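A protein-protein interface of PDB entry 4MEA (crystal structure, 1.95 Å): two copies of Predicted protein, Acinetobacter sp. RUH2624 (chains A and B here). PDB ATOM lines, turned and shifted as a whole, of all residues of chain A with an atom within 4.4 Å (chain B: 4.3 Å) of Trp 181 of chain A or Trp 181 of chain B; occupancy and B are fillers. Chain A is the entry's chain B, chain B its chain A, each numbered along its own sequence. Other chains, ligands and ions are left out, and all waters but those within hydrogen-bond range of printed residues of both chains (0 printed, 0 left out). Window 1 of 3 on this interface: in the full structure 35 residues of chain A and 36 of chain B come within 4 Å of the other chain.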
ATOM      1  N   PRO A 170       0.697  31.826  -8.699  1.00  0.00           N
ATOM      2  CA  PRO A 170       1.145  32.671  -9.814  1.00  0.00           C
ATOM      3  C   PRO A 170       2.388  32.133 -10.524  1.00  0.00           C
ATOM      4  O   PRO A 170       3.284  31.586  -9.885  1.00  0.00           O
ATOM      5  CB  PRO A 170       1.468  34.012  -9.142  1.00  0.00           C
ATOM      6  CG  PRO A 170       0.901  33.924  -7.741  1.00  0.00           C
ATOM      7  CD  PRO A 170       0.861  32.474  -7.385  1.00  0.00           C
ATOM      8  N   GLY A 171       2.446  32.290 -11.840  1.00  0.00           N
ATOM      9  CA  GLY A 171       3.647  31.925 -12.578  1.00  0.00           C
ATOM     10  C   GLY A 171       4.798  32.887 -12.312  1.00  0.00           C
ATOM     11  O   GLY A 171       5.976  32.509 -12.363  1.00  0.00           O
ATOM     12  N   PRO A 177      10.375  34.148 -10.916  1.00  0.00           N
ATOM     13  CA  PRO A 177       9.543  32.970 -11.158  1.00  0.00           C
ATOM     14  C   PRO A 177       8.810  32.524  -9.897  1.00  0.00           C
ATOM     15  O   PRO A 177       9.445  32.439  -8.845  1.00  0.00           O
ATOM     16  CB  PRO A 177      10.567  31.922 -11.586  1.00  0.00           C
ATOM     17  CG  PRO A 177      11.589  32.725 -12.333  1.00  0.00           C
ATOM     18  CD  PRO A 177      11.670  34.061 -11.619  1.00  0.00           C
ATOM     19  N   GLY A 178       7.508  32.253 -10.013  1.00  0.00           N
ATOM     20  CA  GLY A 178       6.661  31.943  -8.867  1.00  0.00           C
ATOM     21  C   GLY A 178       6.396  30.454  -8.693  1.00  0.00           C
ATOM     22  O   GLY A 178       6.733  29.648  -9.551  1.00  0.00           O
ATOM     23  N   LEU A 179       5.805  30.084  -7.560  1.00  0.00           N
ATOM     24  CA  LEU A 179       5.461  28.690  -7.273  1.00  0.00           C
ATOM     25  C   LEU A 179       4.684  28.020  -8.407  1.00  0.00           C
ATOM     26  O   LEU A 179       4.806  26.815  -8.637  1.00  0.00           O
ATOM     27  CB  LEU A 179       4.625  28.630  -5.989  1.00  0.00           C
ATOM     28  CG  LEU A 179       4.038  27.283  -5.564  1.00  0.00           C
ATOM     29  CD1 LEU A 179       5.162  26.273  -5.333  1.00  0.00           C
ATOM     30  CD2 LEU A 179       3.212  27.465  -4.302  1.00  0.00           C
ATOM     31  N   GLY A 180       3.877  28.808  -9.102  1.00  0.00           N
ATOM     32  CA  GLY A 180       2.961  28.277 -10.094  1.00  0.00           C
ATOM     33  C   GLY A 180       3.578  27.854 -11.421  1.00  0.00           C
ATOM     34  O   GLY A 180       3.028  26.979 -12.103  1.00  0.00           O
ATOM     35  N   TRP A 181       4.703  28.457 -11.805  1.00  0.00           N
ATOM     36  CA  TRP A 181       5.167  28.284 -13.191  1.00  0.00           C
ATOM     37  C   TRP A 181       5.461  26.839 -13.558  1.00  0.00           C
ATOM     38  O   TRP A 181       5.088  26.412 -14.639  1.00  0.00           O
ATOM     39  CB  TRP A 181       6.333  29.222 -13.588  1.00  0.00           C
ATOM     40  CG  TRP A 181       7.707  28.748 -13.174  1.00  0.00           C
ATOM     41  CD1 TRP A 181       8.402  29.125 -12.059  1.00  0.00           C
ATOM     42  CD2 TRP A 181       8.543  27.807 -13.866  1.00  0.00           C
ATOM     43  NE1 TRP A 181       9.614  28.478 -12.013  1.00  0.00           N
ATOM     44  CE2 TRP A 181       9.726  27.661 -13.107  1.00  0.00           C
ATOM     45  CE3 TRP A 181       8.412  27.083 -15.059  1.00  0.00           C
ATOM     46  CZ2 TRP A 181      10.764  26.820 -13.493  1.00  0.00           C
ATOM     47  CZ3 TRP A 181       9.446  26.244 -15.442  1.00  0.00           C
ATOM     48  CH2 TRP A 181      10.607  26.116 -14.656  1.00  0.00           C
ATOM     49  N   HIS A 182       6.090  26.070 -12.667  1.00  0.00           N
ATOM     50  CA  HIS A 182       6.443  24.697 -13.030  1.00  0.00           C
ATOM     51  C   HIS A 182       5.222  23.790 -13.201  1.00  0.00           C
ATOM     52  O   HIS A 182       5.271  22.813 -13.955  1.00  0.00           O
ATOM     53  CB  HIS A 182       7.458  24.080 -12.058  1.00  0.00           C
ATOM     54  CG  HIS A 182       6.861  23.620 -10.760  1.00  0.00           C
ATOM     55  ND1 HIS A 182       6.529  24.491  -9.746  1.00  0.00           N
ATOM     56  CD2 HIS A 182       6.543  22.382 -10.310  1.00  0.00           C
ATOM     57  CE1 HIS A 182       6.028  23.813  -8.729  1.00  0.00           C
ATOM     58  NE2 HIS A 182       6.023  22.530  -9.045  1.00  0.00           N
ATOM     59  N   PHE A 183       4.133  24.093 -12.494  1.00  0.00           N
ATOM     60  CA  PHE A 183       2.894  23.348 -12.704  1.00  0.00           C
ATOM     61  C   PHE A 183       2.422  23.467 -14.156  1.00  0.00           C
ATOM     62  O   PHE A 183       1.832  22.538 -14.709  1.00  0.00           O
ATOM     63  CB  PHE A 183       1.805  23.824 -11.743  1.00  0.00           C
ATOM     64  CG  PHE A 183       2.100  23.513 -10.304  1.00  0.00           C
ATOM     65  CD1 PHE A 183       2.043  22.208  -9.845  1.00  0.00           C
ATOM     66  CD2 PHE A 183       2.422  24.525  -9.409  1.00  0.00           C
ATOM     67  CE1 PHE A 183       2.308  21.904  -8.507  1.00  0.00           C
ATOM     68  CE2 PHE A 183       2.688  24.235  -8.072  1.00  0.00           C
ATOM     69  CZ  PHE A 183       2.627  22.919  -7.621  1.00  0.00           C
ATOM     70  N   GLY A 184       2.692  24.616 -14.767  1.00  0.00           N
ATOM     71  CA  GLY A 184       2.353  24.838 -16.162  1.00  0.00           C
ATOM     72  C   GLY A 184       3.374  24.255 -17.135  1.00  0.00           C
ATOM     73  O   GLY A 184       2.999  23.599 -18.096  1.00  0.00           O
ATOM     74  N   TYR A 185       4.662  24.491 -16.903  1.00  0.00           N
ATOM     75  CA  TYR A 185       5.692  23.945 -17.802  1.00  0.00           C
ATOM     76  C   TYR A 185       5.646  22.421 -17.838  1.00  0.00           C
ATOM     77  O   TYR A 185       5.765  21.812 -18.905  1.00  0.00           O
ATOM     78  CB  TYR A 185       7.079  24.420 -17.359  1.00  0.00           C
ATOM     79  CG  TYR A 185       8.252  23.863 -18.149  1.00  0.00           C
ATOM     80  CD1 TYR A 185       8.287  23.944 -19.535  1.00  0.00           C
ATOM     81  CD2 TYR A 185       9.345  23.296 -17.495  1.00  0.00           C
ATOM     82  CE1 TYR A 185       9.376  23.460 -20.255  1.00  0.00           C
ATOM     83  CE2 TYR A 185      10.428  22.803 -18.198  1.00  0.00           C
ATOM     84  CZ  TYR A 185      10.441  22.889 -19.584  1.00  0.00           C
ATOM     85  OH  TYR A 185      11.518  22.403 -20.303  1.00  0.00           O
ATOM     86  N   PHE A 188       2.759  21.024 -20.038  1.00  0.00           N
ATOM     87  CA  PHE A 188       2.698  21.666 -21.355  1.00  0.00           C
ATOM     88  C   PHE A 188       3.118  20.653 -22.422  1.00  0.00           C
ATOM     89  O   PHE A 188       4.290  20.567 -22.762  1.00  0.00           O
ATOM     90  CB  PHE A 188       3.655  22.865 -21.331  1.00  0.00           C
ATOM     91  CG  PHE A 188       3.629  23.731 -22.566  1.00  0.00           C
ATOM     92  CD1 PHE A 188       2.485  24.429 -22.930  1.00  0.00           C
ATOM     93  CD2 PHE A 188       4.786  23.907 -23.325  1.00  0.00           C
ATOM     94  CE1 PHE A 188       2.484  25.263 -24.049  1.00  0.00           C
ATOM     95  CE2 PHE A 188       4.787  24.737 -24.440  1.00  0.00           C
ATOM     96  CZ  PHE A 188       3.632  25.418 -24.795  1.00  0.00           C
ATOM     97  N   TYR A 211      15.643  25.540  -5.325  1.00  0.00           N
ATOM     98  CA  TYR A 211      14.705  25.274  -4.245  1.00  0.00           C
ATOM     99  C   TYR A 211      15.394  24.797  -2.960  1.00  0.00           C
ATOM    100  O   TYR A 211      14.742  24.538  -1.952  1.00  0.00           O
ATOM    101  CB  TYR A 211      13.590  24.343  -4.728  1.00  0.00           C
ATOM    102  CG  TYR A 211      12.792  24.934  -5.887  1.00  0.00           C
ATOM    103  CD1 TYR A 211      11.659  25.706  -5.655  1.00  0.00           C
ATOM    104  CD2 TYR A 211      13.181  24.729  -7.206  1.00  0.00           C
ATOM    105  CE1 TYR A 211      10.930  26.248  -6.705  1.00  0.00           C
ATOM    106  CE2 TYR A 211      12.461  25.268  -8.262  1.00  0.00           C
ATOM    107  CZ  TYR A 211      11.336  26.026  -8.002  1.00  0.00           C
ATOM    108  OH  TYR A 211      10.607  26.559  -9.042  1.00  0.00           O
ATOM    109  N   PRO B 170      -2.151  32.745 -13.128  1.00  0.00           N
ATOM    110  CA  PRO B 170      -1.816  31.420 -12.597  1.00  0.00           C
ATOM    111  C   PRO B 170      -0.960  30.570 -13.544  1.00  0.00           C
ATOM    112  O   PRO B 170      -1.075  30.667 -14.770  1.00  0.00           O
ATOM    113  CB  PRO B 170      -3.188  30.773 -12.379  1.00  0.00           C
ATOM    114  CG  PRO B 170      -4.072  31.421 -13.377  1.00  0.00           C
ATOM    115  CD  PRO B 170      -3.567  32.844 -13.533  1.00  0.00           C
ATOM    116  N   GLY B 171      -0.094  29.740 -12.976  1.00  0.00           N
ATOM    117  CA  GLY B 171       0.717  28.859 -13.797  1.00  0.00           C
ATOM    118  C   GLY B 171      -0.088  27.690 -14.329  1.00  0.00           C
ATOM    119  O   GLY B 171       0.239  27.108 -15.371  1.00  0.00           O
ATOM    120  N   PRO B 177      -1.999  24.196 -18.599  1.00  0.00           N
ATOM    121  CA  PRO B 177      -1.060  25.305 -18.351  1.00  0.00           C
ATOM    122  C   PRO B 177      -1.734  26.670 -18.490  1.00  0.00           C
ATOM    123  O   PRO B 177      -2.477  26.900 -19.444  1.00  0.00           O
ATOM    124  CB  PRO B 177      -0.001  25.109 -19.441  1.00  0.00           C
ATOM    125  CG  PRO B 177       0.004  23.617 -19.661  1.00  0.00           C
ATOM    126  CD  PRO B 177      -1.451  23.202 -19.544  1.00  0.00           C
ATOM    127  N   GLY B 178      -1.486  27.563 -17.537  1.00  0.00           N
ATOM    128  CA  GLY B 178      -2.146  28.855 -17.523  1.00  0.00           C
ATOM    129  C   GLY B 178      -1.338  29.995 -18.111  1.00  0.00           C
ATOM    130  O   GLY B 178      -0.149  29.837 -18.440  1.00  0.00           O
ATOM    131  N   LEU B 179      -1.995  31.147 -18.246  1.00  0.00           N
ATOM    132  CA  LEU B 179      -1.369  32.367 -18.774  1.00  0.00           C
ATOM    133  C   LEU B 179      -0.078  32.734 -18.039  1.00  0.00           C
ATOM    134  O   LEU B 179       0.840  33.330 -18.614  1.00  0.00           O
ATOM    135  CB  LEU B 179      -2.356  33.537 -18.683  1.00  0.00           C
ATOM    136  CG  LEU B 179      -1.860  34.908 -19.145  1.00  0.00           C
ATOM    137  CD1 LEU B 179      -1.438  34.871 -20.606  1.00  0.00           C
ATOM    138  CD2 LEU B 179      -2.934  35.966 -18.910  1.00  0.00           C
ATOM    139  N   GLY B 180      -0.008  32.389 -16.761  1.00  0.00           N
ATOM    140  CA  GLY B 180       1.142  32.757 -15.962  1.00  0.00           C
ATOM    141  C   GLY B 180       2.408  31.947 -16.183  1.00  0.00           C
ATOM    142  O   GLY B 180       3.501  32.446 -15.909  1.00  0.00           O
ATOM    143  N   TRP B 181       2.287  30.705 -16.654  1.00  0.00           N
ATOM    144  CA  TRP B 181       3.439  29.791 -16.594  1.00  0.00           C
ATOM    145  C   TRP B 181       4.643  30.279 -17.398  1.00  0.00           C
ATOM    146  O   TRP B 181       5.785  30.206 -16.923  1.00  0.00           O
ATOM    147  CB  TRP B 181       3.075  28.327 -16.935  1.00  0.00           C
ATOM    148  CG  TRP B 181       3.117  27.948 -18.409  1.00  0.00           C
ATOM    149  CD1 TRP B 181       2.046  27.850 -19.264  1.00  0.00           C
ATOM    150  CD2 TRP B 181       4.280  27.595 -19.186  1.00  0.00           C
ATOM    151  NE1 TRP B 181       2.473  27.485 -20.524  1.00  0.00           N
ATOM    152  CE2 TRP B 181       3.836  27.315 -20.502  1.00  0.00           C
ATOM    153  CE3 TRP B 181       5.650  27.496 -18.900  1.00  0.00           C
ATOM    154  CZ2 TRP B 181       4.712  26.952 -21.526  1.00  0.00           C
ATOM    155  CZ3 TRP B 181       6.519  27.131 -19.920  1.00  0.00           C
ATOM    156  CH2 TRP B 181       6.045  26.862 -21.219  1.00  0.00           C
ATOM    157  N   HIS B 182       4.412  30.813 -18.591  1.00  0.00           N
ATOM    158  CA  HIS B 182       5.561  31.213 -19.390  1.00  0.00           C
ATOM    159  C   HIS B 182       6.284  32.442 -18.815  1.00  0.00           C
ATOM    160  O   HIS B 182       7.480  32.603 -19.033  1.00  0.00           O
ATOM    161  CB  HIS B 182       5.204  31.387 -20.870  1.00  0.00           C
ATOM    162  CG  HIS B 182       4.522  32.681 -21.185  1.00  0.00           C
ATOM    163  ND1 HIS B 182       3.206  32.926 -20.860  1.00  0.00           N
ATOM    164  CD2 HIS B 182       4.974  33.800 -21.798  1.00  0.00           C
ATOM    165  CE1 HIS B 182       2.878  34.143 -21.256  1.00  0.00           C
ATOM    166  NE2 HIS B 182       3.932  34.693 -21.832  1.00  0.00           N
ATOM    167  N   PHE B 183       5.582  33.290 -18.068  1.00  0.00           N
ATOM    168  CA  PHE B 183       6.250  34.436 -17.461  1.00  0.00           C
ATOM    169  C   PHE B 183       7.306  33.952 -16.463  1.00  0.00           C
ATOM    170  O   PHE B 183       8.343  34.600 -16.276  1.00  0.00           O
ATOM    171  CB  PHE B 183       5.259  35.395 -16.780  1.00  0.00           C
ATOM    172  CG  PHE B 183       4.310  36.084 -17.732  1.00  0.00           C
ATOM    173  CD1 PHE B 183       4.741  37.132 -18.532  1.00  0.00           C
ATOM    174  CD2 PHE B 183       2.975  35.709 -17.798  1.00  0.00           C
ATOM    175  CE1 PHE B 183       3.867  37.783 -19.401  1.00  0.00           C
ATOM    176  CE2 PHE B 183       2.099  36.358 -18.660  1.00  0.00           C
ATOM    177  CZ  PHE B 183       2.551  37.402 -19.463  1.00  0.00           C
ATOM    178  N   GLY B 184       7.047  32.804 -15.837  1.00  0.00           N
ATOM    179  CA  GLY B 184       8.007  32.202 -14.925  1.00  0.00           C
ATOM    180  C   GLY B 184       9.122  31.458 -15.639  1.00  0.00           C
ATOM    181  O   GLY B 184      10.307  31.672 -15.364  1.00  0.00           O
ATOM    182  N   TYR B 185       8.752  30.562 -16.548  1.00  0.00           N
ATOM    183  CA  TYR B 185       9.748  29.778 -17.283  1.00  0.00           C
ATOM    184  C   TYR B 185      10.737  30.686 -18.021  1.00  0.00           C
ATOM    185  O   TYR B 185      11.950  30.459 -17.975  1.00  0.00           O
ATOM    186  CB  TYR B 185       9.057  28.815 -18.259  1.00  0.00           C
ATOM    187  CG  TYR B 185       9.994  28.014 -19.159  1.00  0.00           C
ATOM    188  CD1 TYR B 185      11.008  27.214 -18.624  1.00  0.00           C
ATOM    189  CD2 TYR B 185       9.832  28.026 -20.531  1.00  0.00           C
ATOM    190  CE1 TYR B 185      11.844  26.462 -19.451  1.00  0.00           C
ATOM    191  CE2 TYR B 185      10.664  27.279 -21.369  1.00  0.00           C
ATOM    192  CZ  TYR B 185      11.667  26.508 -20.824  1.00  0.00           C
ATOM    193  OH  TYR B 185      12.481  25.762 -21.650  1.00  0.00           O
ATOM    194  N   PHE B 188      13.375  32.239 -15.675  1.00  0.00           N
ATOM    195  CA  PHE B 188      13.993  31.258 -14.778  1.00  0.00           C
ATOM    196  C   PHE B 188      15.442  31.068 -15.212  1.00  0.00           C
ATOM    197  O   PHE B 188      15.732  30.225 -16.048  1.00  0.00           O
ATOM    198  CB  PHE B 188      13.204  29.942 -14.881  1.00  0.00           C
ATOM    199  CG  PHE B 188      13.561  28.886 -13.849  1.00  0.00           C
ATOM    200  CD1 PHE B 188      13.288  29.078 -12.507  1.00  0.00           C
ATOM    201  CD2 PHE B 188      14.097  27.662 -14.249  1.00  0.00           C
ATOM    202  CE1 PHE B 188      13.579  28.092 -11.570  1.00  0.00           C
ATOM    203  CE2 PHE B 188      14.383  26.673 -13.324  1.00  0.00           C
ATOM    204  CZ  PHE B 188      14.125  26.890 -11.976  1.00  0.00           C
ATOM    205  N   TYR B 211      -1.223  28.349 -28.997  1.00  0.00           N
ATOM    206  CA  TYR B 211      -1.929  29.603 -28.802  1.00  0.00           C
ATOM    207  C   TYR B 211      -2.693  30.037 -30.052  1.00  0.00           C
ATOM    208  O   TYR B 211      -3.426  31.024 -30.020  1.00  0.00           O
ATOM    209  CB  TYR B 211      -0.994  30.668 -28.227  1.00  0.00           C
ATOM    210  CG  TYR B 211      -0.322  30.160 -26.969  1.00  0.00           C
ATOM    211  CD1 TYR B 211      -1.042  29.989 -25.792  1.00  0.00           C
ATOM    212  CD2 TYR B 211       1.015  29.807 -26.970  1.00  0.00           C
ATOM    213  CE1 TYR B 211      -0.436  29.501 -24.644  1.00  0.00           C
ATOM    214  CE2 TYR B 211       1.629  29.318 -25.830  1.00  0.00           C
ATOM    215  CZ  TYR B 211       0.902  29.169 -24.677  1.00  0.00           C
ATOM    216  OH  TYR B 211       1.524  28.691 -23.555  1.00  0.00           O
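O of Pro 170 of chain B lies within hydrogen-bond range of N of Gly 180 of chain B (2.8 Å). The backbone carbonyl oxygen (O) of Gly 171 of chain B lies within hydrogen-bond range of the backbone NH (N) of Gly 178 of chain B (2.8 Å). The indole nitrogen (NE1) of Trp 181 of chain B sits at hydrogen-bond distance from the side-chain hydroxyl (OH) of Tyr 211 of chain B (3.4 Å). O of Pro 170 of chain A sits at hydrogen-bond distance from N of Gly 180 of chain A (2.9 Å). The backbone carbonyl oxygen of Gly 171 of chain A lies within hydrogen-bond range of the backbone NH of Gly 178 of chain A (2.8 Å).
Among the printed residues, merely in contact across the chains: Gly 171 of chain A with Gly 171 of chain B, Gly 171 of chain A with Gly 180 of chain B, Gly 171 of chain A with Gly 184 of chain B, Pro 177 of chain A with Gly 184 of chain B, Pro 177 of chain A with Phe 188 of chain B, Gly 180 of chain A with Gly 171 of chain B, Trp 181 of chain A with Trp 181 of chain B, Trp 181 of chain A with Gly 184 of chain B, Trp 181 of chain A with Tyr 185 of chain B, Trp 181 of chain A with Phe 188 of chain B, Gly 184 of chain A with Gly 171 of chain B, Gly 184 of chain A with Pro 177 of chain B, Gly 184 of chain A with Trp 181 of chain B, Tyr 185 of chain A with Trp 181 of chain B, Tyr 185 of chain A with Tyr 185 of chain B, Phe 188 of chain A with Pro 177 of chain B, Phe 188 of chain A with Trp 181 of chain B and Phe 188 of chain A with Tyr 211 of chain B.
Printed residues of chain B within 4 Å of Gly 180 of chain A: Gly 171. Trp 181 of chain A touches just these residues of chain B: Trp 181, Gly 184, Tyr 185 and Phe 188. Of the printed residues of chain B, Gly 184 of chain A touches Gly 171, Pro 177 and Trp 181. Printed residues of chain B within 4 Å of Tyr 185 of chain A: Trp 181 (3.7 Å) and Tyr 185 (3.7 Å). Printed residues of chain B within 4 Å of Phe 188 of chain A: Pro 177 (3.7 Å), Trp 181 (3.5 Å) and Tyr 211 (3.6 Å). The nearest printed residue of chain A that does not touch Trp 181 of chain B is Gly 171 of chain A (4.5 Å). The nearest printed residue of chain A that does not touch Phe 188 of chain B is Tyr 211 of chain A (4.2 Å).
Of the 13 printed residues of chain B, 8 touch a printed residue of chain A. Hydrophobic or aromatic side chains of chain B within 4 Å of the printed part of chain A: Pro 177, Trp 181, Tyr 185, Phe 188 and Tyr 211. Hydrophobic or aromatic side chains of chain A within 4 Å of the printed part of chain B: Pro 177, Trp 181, Tyr 185 and Phe 188. Among the printed residues, 18 pairs touch across the chains.
Gly 171 of chain A touches Gly 180 of chain B, and with the chains exchanged Gly 180 of chain A touches Gly 171 of chain B. Gly 171 of chain A touches Gly 184 of chain B, and with the chains exchanged Gly 184 of chain A touches Gly 171 of chain B. Pro 177 of chain A touches Phe 188 of chain B, and with the chains exchanged Phe 188 of chain A touches Pro 177 of chain B. Tyr 185 of chain B touches its own counterpart, Tyr 185 of chain A.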
